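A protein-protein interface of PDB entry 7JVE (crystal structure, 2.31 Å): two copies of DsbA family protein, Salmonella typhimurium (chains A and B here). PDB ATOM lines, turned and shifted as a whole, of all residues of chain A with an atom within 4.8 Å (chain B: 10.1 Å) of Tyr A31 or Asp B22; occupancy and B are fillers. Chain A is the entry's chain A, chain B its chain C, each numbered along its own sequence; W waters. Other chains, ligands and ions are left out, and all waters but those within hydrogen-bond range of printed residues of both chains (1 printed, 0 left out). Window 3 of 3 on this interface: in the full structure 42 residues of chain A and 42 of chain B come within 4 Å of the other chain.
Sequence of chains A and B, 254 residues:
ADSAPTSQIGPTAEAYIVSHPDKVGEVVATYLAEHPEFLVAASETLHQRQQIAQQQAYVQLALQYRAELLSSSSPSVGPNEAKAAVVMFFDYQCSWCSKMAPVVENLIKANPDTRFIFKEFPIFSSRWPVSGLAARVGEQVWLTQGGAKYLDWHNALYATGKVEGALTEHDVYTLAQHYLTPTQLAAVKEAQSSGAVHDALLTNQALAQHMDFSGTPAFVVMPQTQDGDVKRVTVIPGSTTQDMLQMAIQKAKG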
ATOM      1  N   VAL A  27      20.770  17.521   8.856  1.00  0.00           N
ATOM      2  CA  VAL A  27      20.789  16.188   8.264  1.00  0.00           C
ATOM      3  C   VAL A  27      19.370  15.748   7.906  1.00  0.00           C
ATOM      4  O   VAL A  27      19.130  15.195   6.829  1.00  0.00           O
ATOM      5  CB  VAL A  27      21.494  15.187   9.202  1.00  0.00           C
ATOM      6  CG1 VAL A  27      20.694  14.950  10.468  1.00  0.00           C
ATOM      7  CG2 VAL A  27      21.788  13.912   8.479  1.00  0.00           C
ATOM      8  N   VAL A  28      18.400  16.021   8.780  1.00  0.00           N
ATOM      9  CA  VAL A  28      17.026  15.641   8.472  1.00  0.00           C
ATOM     10  C   VAL A  28      16.458  16.507   7.351  1.00  0.00           C
ATOM     11  O   VAL A  28      15.726  16.014   6.482  1.00  0.00           O
ATOM     12  CB  VAL A  28      16.154  15.708   9.737  1.00  0.00           C
ATOM     13  CG1 VAL A  28      14.670  15.479   9.384  1.00  0.00           C
ATOM     14  CG2 VAL A  28      16.630  14.698  10.771  1.00  0.00           C
ATOM     15  N   ALA A  29      16.765  17.811   7.354  1.00  0.00           N
ATOM     16  CA  ALA A  29      16.288  18.674   6.275  1.00  0.00           C
ATOM     17  C   ALA A  29      16.840  18.220   4.933  1.00  0.00           C
ATOM     18  O   ALA A  29      16.127  18.215   3.921  1.00  0.00           O
ATOM     19  CB  ALA A  29      16.668  20.131   6.536  1.00  0.00           C
ATOM     20  N   THR A  30      18.109  17.817   4.911  1.00  0.00           N
ATOM     21  CA  THR A  30      18.691  17.275   3.692  1.00  0.00           C
ATOM     22  C   THR A  30      17.962  16.004   3.262  1.00  0.00           C
ATOM     23  O   THR A  30      17.600  15.851   2.088  1.00  0.00           O
ATOM     24  CB  THR A  30      20.177  17.008   3.919  1.00  0.00           C
ATOM     25  OG1 THR A  30      20.856  18.261   4.044  1.00  0.00           O
ATOM     26  CG2 THR A  30      20.759  16.248   2.756  1.00  0.00           C
ATOM     27  N   TYR A  31      17.736  15.079   4.203  1.00  0.00           N
ATOM     28  CA  TYR A  31      16.939  13.894   3.904  1.00  0.00           C
ATOM     29  C   TYR A  31      15.598  14.266   3.282  1.00  0.00           C
ATOM     30  O   TYR A  31      15.129  13.606   2.348  1.00  0.00           O
ATOM     31  CB  TYR A  31      16.715  13.066   5.170  1.00  0.00           C
ATOM     32  CG  TYR A  31      15.681  11.964   5.013  1.00  0.00           C
ATOM     33  CD1 TYR A  31      14.323  12.238   5.119  1.00  0.00           C
ATOM     34  CD2 TYR A  31      16.063  10.648   4.776  1.00  0.00           C
ATOM     35  CE1 TYR A  31      13.373  11.236   4.978  1.00  0.00           C
ATOM     36  CE2 TYR A  31      15.120   9.633   4.640  1.00  0.00           C
ATOM     37  CZ  TYR A  31      13.773   9.936   4.741  1.00  0.00           C
ATOM     38  OH  TYR A  31      12.820   8.945   4.606  1.00  0.00           O
ATOM     39  N   LEU A  32      14.960  15.318   3.798  1.00  0.00           N
ATOM     40  CA  LEU A  32      13.631  15.687   3.327  1.00  0.00           C
ATOM     41  C   LEU A  32      13.685  16.322   1.946  1.00  0.00           C
ATOM     42  O   LEU A  32      12.779  16.125   1.128  1.00  0.00           O
ATOM     43  CB  LEU A  32      12.981  16.635   4.320  1.00  0.00           C
ATOM     44  CG  LEU A  32      12.748  15.984   5.662  1.00  0.00           C
ATOM     45  CD1 LEU A  32      12.489  17.078   6.708  1.00  0.00           C
ATOM     46  CD2 LEU A  32      11.573  15.046   5.505  1.00  0.00           C
ATOM     47  N   ALA A  33      14.724  17.111   1.677  1.00  0.00           N
ATOM     48  CA  ALA A  33      14.887  17.656   0.337  1.00  0.00           C
ATOM     49  C   ALA A  33      15.012  16.537  -0.691  1.00  0.00           C
ATOM     50  O   ALA A  33      14.598  16.710  -1.846  1.00  0.00           O
ATOM     51  CB  ALA A  33      16.103  18.582   0.298  1.00  0.00           C
ATOM     52  N   GLU A  34      15.540  15.378  -0.275  1.00  0.00           N
ATOM     53  CA  GLU A  34      15.777  14.236  -1.154  1.00  0.00           C
ATOM     54  C   GLU A  34      14.618  13.246  -1.172  1.00  0.00           C
ATOM     55  O   GLU A  34      14.519  12.445  -2.107  1.00  0.00           O
ATOM     56  CB  GLU A  34      17.060  13.494  -0.741  1.00  0.00           C
ATOM     57  CG  GLU A  34      18.361  14.236  -1.076  1.00  0.00           C
ATOM     58  CD  GLU A  34      19.583  13.722  -0.299  1.00  0.00           C
ATOM     59  OE1 GLU A  34      20.646  14.392  -0.342  1.00  0.00           O
ATOM     60  OE2 GLU A  34      19.493  12.637   0.330  1.00  0.00           O
ATOM     61  N   HIS A  35      13.751  13.266  -0.161  1.00  0.00           N
ATOM     62  CA  HIS A  35      12.493  12.527  -0.172  1.00  0.00           C
ATOM     63  C   HIS A  35      11.365  13.541  -0.028  1.00  0.00           C
ATOM     64  O   HIS A  35      10.687  13.585   1.007  1.00  0.00           O
ATOM     65  CB  HIS A  35      12.419  11.491   0.946  1.00  0.00           C
ATOM     66  CG  HIS A  35      13.616  10.595   1.038  1.00  0.00           C
ATOM     67  ND1 HIS A  35      14.884  11.064   1.310  1.00  0.00           N
ATOM     68  CD2 HIS A  35      13.727   9.249   0.939  1.00  0.00           C
ATOM     69  CE1 HIS A  35      15.730  10.050   1.351  1.00  0.00           C
ATOM     70  NE2 HIS A  35      15.051   8.937   1.139  1.00  0.00           N
ATOM     71  N   TYR B  16      25.209   9.828  15.865  1.00  0.00           N
ATOM     72  CA  TYR B  16      24.682   8.573  15.328  1.00  0.00           C
ATOM     73  C   TYR B  16      23.502   8.818  14.391  1.00  0.00           C
ATOM     74  O   TYR B  16      23.344   8.109  13.392  1.00  0.00           O
ATOM     75  CB  TYR B  16      24.278   7.644  16.477  1.00  0.00           C
ATOM     76  CG  TYR B  16      23.753   6.282  16.053  1.00  0.00           C
ATOM     77  CD1 TYR B  16      24.612   5.197  15.920  1.00  0.00           C
ATOM     78  CD2 TYR B  16      22.399   6.081  15.800  1.00  0.00           C
ATOM     79  CE1 TYR B  16      24.146   3.953  15.545  1.00  0.00           C
ATOM     80  CE2 TYR B  16      21.919   4.835  15.423  1.00  0.00           C
ATOM     81  CZ  TYR B  16      22.799   3.777  15.300  1.00  0.00           C
ATOM     82  OH  TYR B  16      22.343   2.534  14.927  1.00  0.00           O
ATOM     83  N   ILE B  17      22.656   9.803  14.705  1.00  0.00           N
ATOM     84  CA  ILE B  17      21.579  10.173  13.787  1.00  0.00           C
ATOM     85  C   ILE B  17      22.137  10.854  12.545  1.00  0.00           C
ATOM     86  O   ILE B  17      21.658  10.626  11.430  1.00  0.00           O
ATOM     87  CB  ILE B  17      20.542  11.068  14.489  1.00  0.00           C
ATOM     88  CG1 ILE B  17      19.853  10.314  15.623  1.00  0.00           C
ATOM     89  CG2 ILE B  17      19.543  11.626  13.478  1.00  0.00           C
ATOM     90  CD1 ILE B  17      19.509  11.192  16.789  1.00  0.00           C
ATOM     91  N   VAL B  18      23.141  11.714  12.714  1.00  0.00           N
ATOM     92  CA  VAL B  18      23.739  12.372  11.558  1.00  0.00           C
ATOM     93  C   VAL B  18      24.239  11.335  10.560  1.00  0.00           C
ATOM     94  O   VAL B  18      24.094  11.501   9.342  1.00  0.00           O
ATOM     95  CB  VAL B  18      24.858  13.321  12.018  1.00  0.00           C
ATOM     96  CG1 VAL B  18      25.739  13.699  10.851  1.00  0.00           C
ATOM     97  CG2 VAL B  18      24.255  14.559  12.673  1.00  0.00           C
ATOM     98  N   SER B  19      24.808  10.235  11.068  1.00  0.00           N
ATOM     99  CA  SER B  19      25.316   9.139  10.246  1.00  0.00           C
ATOM    100  C   SER B  19      24.200   8.281   9.668  1.00  0.00           C
ATOM    101  O   SER B  19      24.367   7.684   8.598  1.00  0.00           O
ATOM    102  CB  SER B  19      26.225   8.245  11.083  1.00  0.00           C
ATOM    103  OG  SER B  19      27.458   8.878  11.322  1.00  0.00           O
ATOM    104  N   HIS B  20      23.080   8.191  10.372  1.00  0.00           N
ATOM    105  CA  HIS B  20      22.015   7.237  10.080  1.00  0.00           C
ATOM    106  C   HIS B  20      20.702   7.994  10.135  1.00  0.00           C
ATOM    107  O   HIS B  20      19.872   7.768  11.027  1.00  0.00           O
ATOM    108  CB  HIS B  20      22.051   6.087  11.081  1.00  0.00           C
ATOM    109  CG  HIS B  20      23.409   5.483  11.229  1.00  0.00           C
ATOM    110  ND1 HIS B  20      24.126   5.541  12.405  1.00  0.00           N
ATOM    111  CD2 HIS B  20      24.177   4.792  10.352  1.00  0.00           C
ATOM    112  CE1 HIS B  20      25.280   4.919  12.244  1.00  0.00           C
ATOM    113  NE2 HIS B  20      25.337   4.458  11.006  1.00  0.00           N
ATOM    114  N   PRO B  21      20.488   8.916   9.190  1.00  0.00           N
ATOM    115  CA  PRO B  21      19.379   9.875   9.316  1.00  0.00           C
ATOM    116  C   PRO B  21      18.016   9.339   8.906  1.00  0.00           C
ATOM    117  O   PRO B  21      17.005   9.998   9.197  1.00  0.00           O
ATOM    118  CB  PRO B  21      19.811  11.016   8.385  1.00  0.00           C
ATOM    119  CG  PRO B  21      20.667  10.333   7.340  1.00  0.00           C
ATOM    120  CD  PRO B  21      21.359   9.204   8.033  1.00  0.00           C
ATOM    121  N   ASP B  22      17.948   8.166   8.276  1.00  0.00           N
ATOM    122  CA  ASP B  22      16.760   7.806   7.500  1.00  0.00           C
ATOM    123  C   ASP B  22      15.543   7.554   8.385  1.00  0.00           C
ATOM    124  O   ASP B  22      14.431   7.989   8.058  1.00  0.00           O
ATOM    125  CB  ASP B  22      17.041   6.568   6.632  1.00  0.00           C
ATOM    126  CG  ASP B  22      17.899   6.880   5.403  1.00  0.00           C
ATOM    127  OD1 ASP B  22      18.329   8.040   5.230  1.00  0.00           O
ATOM    128  OD2 ASP B  22      18.111   5.961   4.584  1.00  0.00           O
ATOM    129  N   LYS B  23      15.711   6.817   9.485  1.00  0.00           N
ATOM    130  CA  LYS B  23      14.544   6.466  10.290  1.00  0.00           C
ATOM    131  C   LYS B  23      13.976   7.686  11.006  1.00  0.00           C
ATOM    132  O   LYS B  23      12.756   7.823  11.130  1.00  0.00           O
ATOM    133  CB  LYS B  23      14.908   5.360  11.272  1.00  0.00           C
ATOM    134  CG  LYS B  23      15.171   4.034  10.582  1.00  0.00           C
ATOM    135  CD  LYS B  23      15.501   2.967  11.595  1.00  0.00           C
ATOM    136  CE  LYS B  23      16.327   1.847  10.995  1.00  0.00           C
ATOM    137  NZ  LYS B  23      16.238   0.612  11.836  1.00  0.00           N
ATOM    138  N   VAL B  24      14.835   8.591  11.476  1.00  0.00           N
ATOM    139  CA  VAL B  24      14.337   9.845  12.032  1.00  0.00           C
ATOM    140  C   VAL B  24      13.689  10.685  10.937  1.00  0.00           C
ATOM    141  O   VAL B  24      12.649  11.317  11.154  1.00  0.00           O
ATOM    142  CB  VAL B  24      15.467  10.615  12.748  1.00  0.00           C
ATOM    143  CG1 VAL B  24      14.979  11.981  13.207  1.00  0.00           C
ATOM    144  CG2 VAL B  24      16.003   9.812  13.932  1.00  0.00           C
ATOM    145  N   GLY B  25      14.291  10.701   9.745  1.00  0.00           N
ATOM    146  CA  GLY B  25      13.706  11.442   8.642  1.00  0.00           C
ATOM    147  C   GLY B  25      12.292  10.992   8.332  1.00  0.00           C
ATOM    148  O   GLY B  25      11.410  11.815   8.062  1.00  0.00           O
ATOM    149  N   GLU B  26      12.051   9.679   8.390  1.00  0.00           N
ATOM    150  CA  GLU B  26      10.724   9.155   8.091  1.00  0.00           C
ATOM    151  C   GLU B  26       9.700   9.609   9.125  1.00  0.00           C
ATOM    152  O   GLU B  26       8.601  10.056   8.765  1.00  0.00           O
ATOM    153  CB  GLU B  26      10.774   7.630   7.987  1.00  0.00           C
ATOM    154  CG  GLU B  26      11.468   7.154   6.721  1.00  0.00           C
ATOM    155  CD  GLU B  26      11.971   5.705   6.791  1.00  0.00           C
ATOM    156  OE1 GLU B  26      11.770   5.029   7.826  1.00  0.00           O
ATOM    157  OE2 GLU B  26      12.568   5.238   5.790  1.00  0.00           O
ATOM    158  N   VAL B  27      10.028   9.519  10.417  1.00  0.00           N
ATOM    159  CA  VAL B  27       9.012   9.921  11.385  1.00  0.00           C
ATOM    160  C   VAL B  27       8.832  11.434  11.372  1.00  0.00           C
ATOM    161  O   VAL B  27       7.717  11.923  11.586  1.00  0.00           O
ATOM    162  CB  VAL B  27       9.311   9.387  12.804  1.00  0.00           C
ATOM    163  CG1 VAL B  27       9.241   7.877  12.817  1.00  0.00           C
ATOM    164  CG2 VAL B  27      10.643   9.882  13.311  1.00  0.00           C
ATOM    165  N   VAL B  28       9.901  12.198  11.100  1.00  0.00           N
ATOM    166  CA  VAL B  28       9.760  13.645  10.960  1.00  0.00           C
ATOM    167  C   VAL B  28       8.899  13.979   9.747  1.00  0.00           C
ATOM    168  O   VAL B  28       8.002  14.831   9.825  1.00  0.00           O
ATOM    169  CB  VAL B  28      11.138  14.327  10.877  1.00  0.00           C
ATOM    170  CG1 VAL B  28      10.969  15.806  10.577  1.00  0.00           C
ATOM    171  CG2 VAL B  28      11.903  14.155  12.163  1.00  0.00           C
ATOM    172  N   ALA B  29       9.131  13.303   8.614  1.00  0.00           N
ATOM    173  CA  ALA B  29       8.272  13.509   7.444  1.00  0.00           C
ATOM    174  C   ALA B  29       6.801  13.298   7.794  1.00  0.00           C
ATOM    175  O   ALA B  29       5.941  14.105   7.426  1.00  0.00           O
ATOM    176  CB  ALA B  29       8.683  12.576   6.301  1.00  0.00           C
ATOM    177  N   THR B  30       6.491  12.210   8.512  1.00  0.00           N
ATOM    178  CA  THR B  30       5.127  12.011   9.002  1.00  0.00           C
ATOM    179  C   THR B  30       4.682  13.157   9.914  1.00  0.00           C
ATOM    180  O   THR B  30       3.524  13.601   9.851  1.00  0.00           O
ATOM    181  CB  THR B  30       5.020  10.671   9.734  1.00  0.00           C
ATOM    182  OG1 THR B  30       5.442   9.621   8.857  1.00  0.00           O
ATOM    183  CG2 THR B  30       3.599  10.403  10.158  1.00  0.00           C
ATOM    184  N   TYR B  31       5.588  13.661  10.756  1.00  0.00           N
ATOM    185  CA  TYR B  31       5.228  14.749  11.661  1.00  0.00           C
ATOM    186  C   TYR B  31       4.956  16.037  10.892  1.00  0.00           C
ATOM    187  O   TYR B  31       3.986  16.755  11.173  1.00  0.00           O
ATOM    188  CB  TYR B  31       6.336  14.968  12.691  1.00  0.00           C
ATOM    189  CG  TYR B  31       6.159  16.246  13.475  1.00  0.00           C
ATOM    190  CD1 TYR B  31       6.637  17.458  12.989  1.00  0.00           C
ATOM    191  CD2 TYR B  31       5.503  16.245  14.700  1.00  0.00           C
ATOM    192  CE1 TYR B  31       6.469  18.637  13.707  1.00  0.00           C
ATOM    193  CE2 TYR B  31       5.336  17.421  15.434  1.00  0.00           C
ATOM    194  CZ  TYR B  31       5.817  18.614  14.928  1.00  0.00           C
ATOM    195  OH  TYR B  31       5.652  19.784  15.641  1.00  0.00           O
ATOM    196  N   LEU B  32       5.821  16.356   9.930  1.00  0.00           N
ATOM    197  CA  LEU B  32       5.648  17.571   9.142  1.00  0.00           C
ATOM    198  C   LEU B  32       4.308  17.580   8.404  1.00  0.00           C
ATOM    199  O   LEU B  32       3.661  18.631   8.295  1.00  0.00           O
ATOM    200  CB  LEU B  32       6.809  17.716   8.166  1.00  0.00           C
ATOM    201  CG  LEU B  32       8.146  18.056   8.828  1.00  0.00           C
ATOM    202  CD1 LEU B  32       9.175  18.273   7.746  1.00  0.00           C
ATOM    203  CD2 LEU B  32       8.056  19.299   9.753  1.00  0.00           C
HETATM  204  O   HOH W   1      17.437   6.984   1.661  1.00  0.00           O
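The backbone carbonyl oxygen (O) of Tyr A31 sits at hydrogen-bond distance from a ring nitrogen (ND1) of His A35, at 2.8 Å.
The side-chain hydroxyl (OG1) of Thr B30 is in hydrogen-bond range of the backbone carbonyl oxygen (O) of Glu B26 (3.2 Å).
Among the printed residues, pairs that only touch across the chains: Val A27 with Val B18 (3.4 Å), Val A27 with Pro B21 (3.5 Å), Val A28 with Val B28 (3.9 Å), Tyr A31 with Asp B22 (3.5 Å), Tyr A31 with Gly B25 (3.5 Å), Tyr A31 with Glu B26 (3.1 Å), Leu A32 with Ala B29 (3.9 Å) and Leu A32 with Leu B32 (3.7 Å).
Tyr A31 touches three residues of chain B.
Of chain A, only Tyr A31 (3.5 Å) comes within 4 Å of Asp B22.
No residue of chain B comes within 4 Å of Ala A29.
No residue of chain B comes within 4 Å of Thr A30.
Leu A32 touches just these residues of chain B: Ala B29 and Leu B32.
No residue of chain B comes within 4 Å of Ala A33.
No residue of chain B comes within 4 Å of His A35.
Printed residues of chain A within 4 Å of Gly B25: Tyr A31 (3.5 Å).
Of the printed residues of chain A, Val B18 touches Val A27 (3.4 Å).
Printed residues of chain B within 4 Å of Val A27: Val B18 and Pro B21.
Printed residues of chain B within 4 Å of Val A28: Val B28 (3.9 Å).
Printed residues of chain A within 4 Å of Ala B29: Leu A32.
The nearest residue of chain B that does not touch Tyr A31 is Pro B21 (4.6 Å).
The nearest printed residue of chain A that does not touch Asp B22 is His A35 (5.1 Å).
Of the 9 printed residues of chain A, 4 touch a printed residue of chain B.
Along chain B the printed residues that touch a printed residue of chain A span positions 18 to 32.
Among the printed residues, 8 pairs touch across the chains.
Val B28 touches its own counterpart, Val A28.
Leu A32 touches Ala B29, but with the chains exchanged Ala A29 does not touch Leu B32 (7.3 Å).
Leu A32 touches its own counterpart, Leu B32.
Positions printed for both chains: 27, 28, 29, 30, 31 and 32.
Of the 8 pairs that touch across the chains among the printed residues, 2 have their exchanged pair printed and touching as well.
Water W1 bridges a ring nitrogen (NE2) of His A35 and the side-chain carboxylate of Asp B22.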
